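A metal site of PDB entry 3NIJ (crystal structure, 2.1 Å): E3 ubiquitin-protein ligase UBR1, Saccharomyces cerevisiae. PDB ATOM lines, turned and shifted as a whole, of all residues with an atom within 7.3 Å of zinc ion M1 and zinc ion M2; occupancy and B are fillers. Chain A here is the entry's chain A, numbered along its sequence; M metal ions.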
ATOM      1  N   HIS A   4      30.498   3.929  27.822  1.00  0.00           N
ATOM      2  CA  HIS A   4      29.827   5.143  28.276  1.00  0.00           C
ATOM      3  C   HIS A   4      28.599   4.831  29.118  1.00  0.00           C
ATOM      4  O   HIS A   4      27.917   5.739  29.601  1.00  0.00           O
ATOM      5  CB  HIS A   4      29.456   6.008  27.077  1.00  0.00           C
ATOM      6  CG  HIS A   4      30.530   6.081  26.030  1.00  0.00           C
ATOM      7  ND1 HIS A   4      31.730   6.740  26.239  1.00  0.00           N
ATOM      8  CD2 HIS A   4      30.584   5.576  24.775  1.00  0.00           C
ATOM      9  CE1 HIS A   4      32.472   6.638  25.153  1.00  0.00           C
ATOM     10  NE2 HIS A   4      31.801   5.937  24.250  1.00  0.00           N
ATOM     11  N   LYS A   5      28.317   3.535  29.283  1.00  0.00           N
ATOM     12  CA  LYS A   5      27.253   3.043  30.143  1.00  0.00           C
ATOM     13  C   LYS A   5      27.504   3.469  31.580  1.00  0.00           C
ATOM     14  O   LYS A   5      28.648   3.518  32.033  1.00  0.00           O
ATOM     15  CB  LYS A   5      27.170   1.510  30.074  1.00  0.00           C
ATOM     16  CG  LYS A   5      26.990   0.958  28.670  1.00  0.00           C
ATOM     17  CD  LYS A   5      27.458  -0.492  28.588  1.00  0.00           C
ATOM     18  CE  LYS A   5      27.483  -0.963  27.136  1.00  0.00           C
ATOM     19  NZ  LYS A   5      28.061  -2.317  27.006  1.00  0.00           N
ATOM     20  N   HIS A   6      26.422   3.787  32.297  1.00  0.00           N
ATOM     21  CA  HIS A   6      26.512   4.257  33.678  1.00  0.00           C
ATOM     22  C   HIS A   6      25.293   3.834  34.497  1.00  0.00           C
ATOM     23  O   HIS A   6      24.728   4.625  35.252  1.00  0.00           O
ATOM     24  CB  HIS A   6      26.684   5.785  33.695  1.00  0.00           C
ATOM     25  CG  HIS A   6      25.566   6.523  33.018  1.00  0.00           C
ATOM     26  ND1 HIS A   6      24.456   6.962  33.709  1.00  0.00           N
ATOM     27  CD2 HIS A   6      25.377   6.872  31.728  1.00  0.00           C
ATOM     28  CE1 HIS A   6      23.638   7.561  32.866  1.00  0.00           C
ATOM     29  NE2 HIS A   6      24.175   7.522  31.657  1.00  0.00           N
ATOM     30  N   ARG A   9      23.331   5.244  37.979  1.00  0.00           N
ATOM     31  CA  ARG A   9      23.862   6.539  38.384  1.00  0.00           C
ATOM     32  C   ARG A   9      23.766   7.530  37.226  1.00  0.00           C
ATOM     33  O   ARG A   9      23.455   7.149  36.094  1.00  0.00           O
ATOM     34  CB  ARG A   9      25.298   6.435  38.912  1.00  0.00           C
ATOM     35  CG  ARG A   9      26.292   5.712  37.989  1.00  0.00           C
ATOM     36  CD  ARG A   9      27.736   6.153  38.262  1.00  0.00           C
ATOM     37  NE  ARG A   9      28.030   7.459  37.630  1.00  0.00           N
ATOM     38  CZ  ARG A   9      29.247   8.001  37.552  1.00  0.00           C
ATOM     39  NH1 ARG A   9      30.324   7.366  38.064  1.00  0.00           N
ATOM     40  NH2 ARG A   9      29.402   9.192  36.952  1.00  0.00           N
ATOM     41  N   ASN A  10      24.018   8.802  37.522  1.00  0.00           N
ATOM     42  CA  ASN A  10      24.034   9.838  36.496  1.00  0.00           C
ATOM     43  C   ASN A  10      25.248   9.651  35.588  1.00  0.00           C
ATOM     44  O   ASN A  10      26.250   9.047  35.987  1.00  0.00           O
ATOM     45  CB  ASN A  10      24.070  11.216  37.146  1.00  0.00           C
ATOM     46  CG  ASN A  10      25.382  11.483  37.873  1.00  0.00           C
ATOM     47  OD1 ASN A  10      25.837  10.674  38.693  1.00  0.00           O
ATOM     48  ND2 ASN A  10      26.015  12.607  37.555  1.00  0.00           N
ATOM     49  N   CYS A  11      25.138  10.159  34.358  1.00  0.00           N
ATOM     50  CA  CYS A  11      26.280  10.149  33.451  1.00  0.00           C
ATOM     51  C   CYS A  11      27.372  11.076  33.976  1.00  0.00           C
ATOM     52  O   CYS A  11      28.461  10.618  34.356  1.00  0.00           O
ATOM     53  CB  CYS A  11      25.849  10.530  32.024  1.00  0.00           C
ATOM     54  SG  CYS A  11      27.245  10.573  30.898  1.00  0.00           S
ATOM     55  N   GLY A  12      27.085  12.375  34.006  1.00  0.00           N
ATOM     56  CA  GLY A  12      28.045  13.347  34.539  1.00  0.00           C
ATOM     57  C   GLY A  12      29.266  13.614  33.658  1.00  0.00           C
ATOM     58  O   GLY A  12      30.193  14.312  34.082  1.00  0.00           O
ATOM     59  N   ARG A  13      29.273  13.056  32.452  1.00  0.00           N
ATOM     60  CA  ARG A  13      30.341  13.297  31.467  1.00  0.00           C
ATOM     61  C   ARG A  13      30.457  14.786  31.184  1.00  0.00           C
ATOM     62  O   ARG A  13      29.489  15.428  30.787  1.00  0.00           O
ATOM     63  CB  ARG A  13      30.063  12.544  30.158  1.00  0.00           C
ATOM     64  CG  ARG A  13      31.027  12.854  29.013  1.00  0.00           C
ATOM     65  CD  ARG A  13      30.714  12.011  27.787  1.00  0.00           C
ATOM     66  NE  ARG A  13      31.449  10.747  27.830  1.00  0.00           N
ATOM     67  CZ  ARG A  13      32.647  10.557  27.282  1.00  0.00           C
ATOM     68  NH1 ARG A  13      33.230  11.547  26.617  1.00  0.00           N
ATOM     69  NH2 ARG A  13      33.250   9.373  27.373  1.00  0.00           N
ATOM     70  N   PHE A  15      31.408  17.983  29.148  1.00  0.00           N
ATOM     71  CA  PHE A  15      31.551  18.378  27.751  1.00  0.00           C
ATOM     72  C   PHE A  15      32.868  19.103  27.531  1.00  0.00           C
ATOM     73  O   PHE A  15      33.358  19.823  28.407  1.00  0.00           O
ATOM     74  CB  PHE A  15      30.379  19.246  27.298  1.00  0.00           C
ATOM     75  CG  PHE A  15      29.067  18.539  27.315  1.00  0.00           C
ATOM     76  CD1 PHE A  15      28.696  17.712  26.263  1.00  0.00           C
ATOM     77  CD2 PHE A  15      28.189  18.684  28.391  1.00  0.00           C
ATOM     78  CE1 PHE A  15      27.477  17.035  26.285  1.00  0.00           C
ATOM     79  CE2 PHE A  15      26.964  18.020  28.414  1.00  0.00           C
ATOM     80  CZ  PHE A  15      26.601  17.189  27.366  1.00  0.00           C
ATOM     81  N   VAL A  34      20.814  18.766  29.839  1.00  0.00           N
ATOM     82  CA  VAL A  34      21.512  18.366  28.612  1.00  0.00           C
ATOM     83  C   VAL A  34      21.932  16.892  28.590  1.00  0.00           C
ATOM     84  O   VAL A  34      22.129  16.265  29.641  1.00  0.00           O
ATOM     85  CB  VAL A  34      22.776  19.250  28.335  1.00  0.00           C
ATOM     86  CG1 VAL A  34      22.409  20.720  28.183  1.00  0.00           C
ATOM     87  CG2 VAL A  34      23.808  19.094  29.458  1.00  0.00           C
ATOM     88  N   LEU A  35      22.103  16.364  27.378  1.00  0.00           N
ATOM     89  CA  LEU A  35      22.553  14.989  27.125  1.00  0.00           C
ATOM     90  C   LEU A  35      23.766  14.994  26.200  1.00  0.00           C
ATOM     91  O   LEU A  35      23.841  15.794  25.273  1.00  0.00           O
ATOM     92  CB  LEU A  35      21.444  14.171  26.470  1.00  0.00           C
ATOM     93  CG  LEU A  35      20.176  13.882  27.291  1.00  0.00           C
ATOM     94  CD1 LEU A  35      19.013  13.498  26.394  1.00  0.00           C
ATOM     95  CD2 LEU A  35      20.442  12.802  28.320  1.00  0.00           C
ATOM     96  N   CYS A  36      24.717  14.096  26.453  1.00  0.00           N
ATOM     97  CA  CYS A  36      25.853  13.930  25.546  1.00  0.00           C
ATOM     98  C   CYS A  36      25.486  13.038  24.364  1.00  0.00           C
ATOM     99  O   CYS A  36      24.406  12.430  24.350  1.00  0.00           O
ATOM    100  CB  CYS A  36      27.086  13.404  26.279  1.00  0.00           C
ATOM    101  SG  CYS A  36      26.996  11.678  26.794  1.00  0.00           S
ATOM    102  N   ILE A  37      26.394  12.944  23.386  1.00  0.00           N
ATOM    103  CA  ILE A  37      26.180  12.164  22.169  1.00  0.00           C
ATOM    104  C   ILE A  37      26.100  10.659  22.462  1.00  0.00           C
ATOM    105  O   ILE A  37      25.429   9.919  21.756  1.00  0.00           O
ATOM    106  CB  ILE A  37      27.245  12.506  21.063  1.00  0.00           C
ATOM    107  CG1 ILE A  37      26.803  11.958  19.694  1.00  0.00           C
ATOM    108  CG2 ILE A  37      28.652  12.016  21.466  1.00  0.00           C
ATOM    109  CD1 ILE A  37      27.573  12.514  18.495  1.00  0.00           C
ATOM    110  N   HIS A  38      26.785  10.218  23.518  1.00  0.00           N
ATOM    111  CA  HIS A  38      26.769   8.809  23.900  1.00  0.00           C
ATOM    112  C   HIS A  38      25.489   8.406  24.638  1.00  0.00           C
ATOM    113  O   HIS A  38      25.196   7.208  24.767  1.00  0.00           O
ATOM    114  CB  HIS A  38      27.997   8.480  24.747  1.00  0.00           C
ATOM    115  CG  HIS A  38      29.299   8.840  24.088  1.00  0.00           C
ATOM    116  ND1 HIS A  38      30.163   9.773  24.610  1.00  0.00           N
ATOM    117  CD2 HIS A  38      29.847   8.403  22.929  1.00  0.00           C
ATOM    118  CE1 HIS A  38      31.209   9.892  23.813  1.00  0.00           C
ATOM    119  NE2 HIS A  38      31.043   9.079  22.781  1.00  0.00           N
ATOM    120  N   CYS A  39      24.736   9.401  25.113  1.00  0.00           N
ATOM    121  CA  CYS A  39      23.568   9.167  25.955  1.00  0.00           C
ATOM    122  C   CYS A  39      22.253   9.467  25.214  1.00  0.00           C
ATOM    123  O   CYS A  39      21.248   8.761  25.381  1.00  0.00           O
ATOM    124  CB  CYS A  39      23.660  10.014  27.236  1.00  0.00           C
ATOM    125  SG  CYS A  39      24.976   9.577  28.470  1.00  0.00           S
ATOM    126  N   PHE A  40      22.262  10.523  24.392  1.00  0.00           N
ATOM    127  CA  PHE A  40      21.085  10.921  23.625  1.00  0.00           C
ATOM    128  C   PHE A  40      20.576   9.813  22.698  1.00  0.00           C
ATOM    129  O   PHE A  40      21.304   9.314  21.829  1.00  0.00           O
ATOM    130  CB  PHE A  40      21.350  12.205  22.828  1.00  0.00           C
ATOM    131  CG  PHE A  40      20.184  12.675  21.980  1.00  0.00           C
ATOM    132  CD1 PHE A  40      19.162  13.429  22.533  1.00  0.00           C
ATOM    133  CD2 PHE A  40      20.120  12.351  20.624  1.00  0.00           C
ATOM    134  CE1 PHE A  40      18.088  13.872  21.746  1.00  0.00           C
ATOM    135  CE2 PHE A  40      19.049  12.773  19.830  1.00  0.00           C
ATOM    136  CZ  PHE A  40      18.033  13.536  20.406  1.00  0.00           C
ATOM    137  N   ILE A  62      28.013  19.375  32.295  1.00  0.00           N
ATOM    138  CA  ILE A  62      27.989  17.911  32.340  1.00  0.00           C
ATOM    139  C   ILE A  62      26.674  17.311  31.837  1.00  0.00           C
ATOM    140  O   ILE A  62      25.624  17.943  31.919  1.00  0.00           O
ATOM    141  CB  ILE A  62      28.288  17.359  33.769  1.00  0.00           C
ATOM    142  CG1 ILE A  62      27.249  17.857  34.780  1.00  0.00           C
ATOM    143  CG2 ILE A  62      29.712  17.725  34.210  1.00  0.00           C
ATOM    144  CD1 ILE A  62      27.105  16.997  36.029  1.00  0.00           C
ATOM    145  N   CYS A  63      26.753  16.084  31.339  1.00  0.00           N
ATOM    146  CA  CYS A  63      25.586  15.360  30.851  1.00  0.00           C
ATOM    147  C   CYS A  63      24.666  14.997  32.022  1.00  0.00           C
ATOM    148  O   CYS A  63      25.142  14.578  33.082  1.00  0.00           O
ATOM    149  CB  CYS A  63      26.002  14.101  30.098  1.00  0.00           C
ATOM    150  SG  CYS A  63      24.621  13.047  29.653  1.00  0.00           S
ATOM    151  N   ASP A  64      23.360  15.154  31.818  1.00  0.00           N
ATOM    152  CA  ASP A  64      22.351  14.925  32.853  1.00  0.00           C
ATOM    153  C   ASP A  64      21.626  13.588  32.759  1.00  0.00           C
ATOM    154  O   ASP A  64      20.730  13.300  33.566  1.00  0.00           O
ATOM    155  CB  ASP A  64      21.334  16.074  32.889  1.00  0.00           C
ATOM    156  CG  ASP A  64      21.976  17.399  33.194  1.00  0.00           C
ATOM    157  OD1 ASP A  64      22.701  17.478  34.196  1.00  0.00           O
ATOM    158  OD2 ASP A  64      21.769  18.369  32.433  1.00  0.00           O
ATOM    159  N   CYS A  65      22.024  12.759  31.791  1.00  0.00           N
ATOM    160  CA  CYS A  65      21.429  11.425  31.653  1.00  0.00           C
ATOM    161  C   CYS A  65      21.511  10.653  32.969  1.00  0.00           C
ATOM    162  O   CYS A  65      22.585  10.525  33.563  1.00  0.00           O
ATOM    163  CB  CYS A  65      22.130  10.624  30.562  1.00  0.00           C
ATOM    164  SG  CYS A  65      21.242   9.132  30.090  1.00  0.00           S
ATOM    165  N   GLY A  66      20.373  10.161  33.437  1.00  0.00           N
ATOM    166  CA  GLY A  66      20.309   9.411  34.687  1.00  0.00           C
ATOM    167  C   GLY A  66      20.108  10.245  35.945  1.00  0.00           C
ATOM    168  O   GLY A  66      19.973   9.700  37.035  1.00  0.00           O
ATOM    169  N   HIS A  76      16.065   6.587  28.020  1.00  0.00           N
ATOM    170  CA  HIS A  76      16.667   5.281  27.781  1.00  0.00           C
ATOM    171  C   HIS A  76      18.027   5.482  27.118  1.00  0.00           C
ATOM    172  O   HIS A  76      18.118   5.604  25.890  1.00  0.00           O
ATOM    173  CB  HIS A  76      15.753   4.416  26.901  1.00  0.00           C
ATOM    174  CG  HIS A  76      14.369   4.260  27.444  1.00  0.00           C
ATOM    175  ND1 HIS A  76      14.007   3.212  28.258  1.00  0.00           N
ATOM    176  CD2 HIS A  76      13.256   5.023  27.288  1.00  0.00           C
ATOM    177  CE1 HIS A  76      12.727   3.324  28.578  1.00  0.00           C
ATOM    178  NE2 HIS A  76      12.253   4.422  28.005  1.00  0.00           N
ATOM    179  N   CYS A  77      19.069   5.536  27.959  1.00  0.00           N
ATOM    180  CA  CYS A  77      20.456   5.797  27.555  1.00  0.00           C
ATOM    181  C   CYS A  77      20.848   5.035  26.289  1.00  0.00           C
ATOM    182  O   CYS A  77      20.704   3.805  26.227  1.00  0.00           O
ATOM    183  CB  CYS A  77      21.410   5.422  28.716  1.00  0.00           C
ATOM    184  SG  CYS A  77      22.999   6.324  28.768  1.00  0.00           S
ATOM    185  N   LYS A  78      21.344   5.761  25.290  1.00  0.00           N
ATOM    186  CA  LYS A  78      21.803   5.156  24.033  1.00  0.00           C
ATOM    187  C   LYS A  78      22.968   4.189  24.240  1.00  0.00           C
ATOM    188  O   LYS A  78      23.066   3.168  23.560  1.00  0.00           O
ATOM    189  CB  LYS A  78      22.189   6.223  23.004  1.00  0.00           C
ATOM    190  CG  LYS A  78      22.090   5.746  21.559  1.00  0.00           C
ATOM    191  CD  LYS A  78      23.224   6.283  20.693  1.00  0.00           C
ATOM    192  CE  LYS A  78      23.096   5.785  19.257  1.00  0.00           C
ATOM    193  NZ  LYS A  78      24.409   5.794  18.533  1.00  0.00           N
ATOM    194  N   ALA A  79      23.855   4.517  25.178  1.00  0.00           N
ATOM    195  CA  ALA A  79      24.995   3.652  25.526  1.00  0.00           C
ATOM    196  C   ALA A  79      24.526   2.301  26.096  1.00  0.00           C
ATOM    197  O   ALA A  79      25.226   1.298  25.950  1.00  0.00           O
ATOM    198  CB  ALA A  79      25.917   4.345  26.505  1.00  0.00           C
ATOM    199  N   GLU A  80      23.347   2.303  26.703  1.00  0.00           N
ATOM    200  CA  GLU A  80      22.795   1.125  27.383  1.00  0.00           C
ATOM    201  C   GLU A  80      22.246   0.064  26.417  1.00  0.00           C
ATOM    202  O   GLU A  80      22.059  -1.094  26.805  1.00  0.00           O
ATOM    203  CB  GLU A  80      21.713   1.552  28.371  1.00  0.00           C
ATOM    204  CG  GLU A  80      21.627   0.715  29.635  1.00  0.00           C
ATOM    205  CD  GLU A  80      22.966   0.596  30.348  1.00  0.00           C
ATOM    206  OE1 GLU A  80      23.508   1.640  30.781  1.00  0.00           O
ATOM    207  OE2 GLU A  80      23.461  -0.537  30.482  1.00  0.00           O
HETATM  208 ZN    ZN M   1      25.973  11.336  28.949  1.00  0.00          ZN
HETATM  209 ZN    ZN M   2      23.449   8.069  29.478  1.00  0.00          ZN
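The backbone carbonyl oxygen (O) of Cys 39 is in hydrogen-bond range of the backbone NH (N) of Lys 78 (3.0 Å). SG of Cys 63 lies close to N of Cys 65, 3.4 Å away. N of Cys 63 sits at hydrogen-bond distance from O of Arg 13, at 2.9 Å. The backbone NH (N) of Cys 11 is in hydrogen-bond range of a ring nitrogen (ND1) of His 6, 3.3 Å away. The backbone carbonyl oxygen of Arg 9 is in hydrogen-bond range of a ring nitrogen (ND1) of His 6 (2.6 Å). SG of Cys 36 lies close to N of His 38, 3.6 Å away. The backbone carbonyl oxygen of Cys 65 is in hydrogen-bond range of the backbone NH of Cys 11. The backbone carbonyl oxygen (O) of Cys 11 sits at hydrogen-bond distance from the guanidinium group (NH2) of Arg 9.
Zinc ion M1 is bound by the side-chain sulfur (SG) of Cys 39 (2.1 Å), the side-chain sulfur (SG) of Cys 63 (2.3 Å), the side-chain sulfur (SG) of Cys 36 (2.4 Å) and the side-chain sulfur (SG) of Cys 11 (2.4 Å).
Zinc ion M2 is bound by SG of Cys 77 (1.9 Å), NE2 of His 6 (2.4 Å), SG of Cys 39 (2.4 Å) and SG of Cys 65 (2.5 Å). Zinc ion M2 has four donor atoms within binding distance.
Of the 26 residues printed, 4 come within 4 Å of zinc ion M2.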
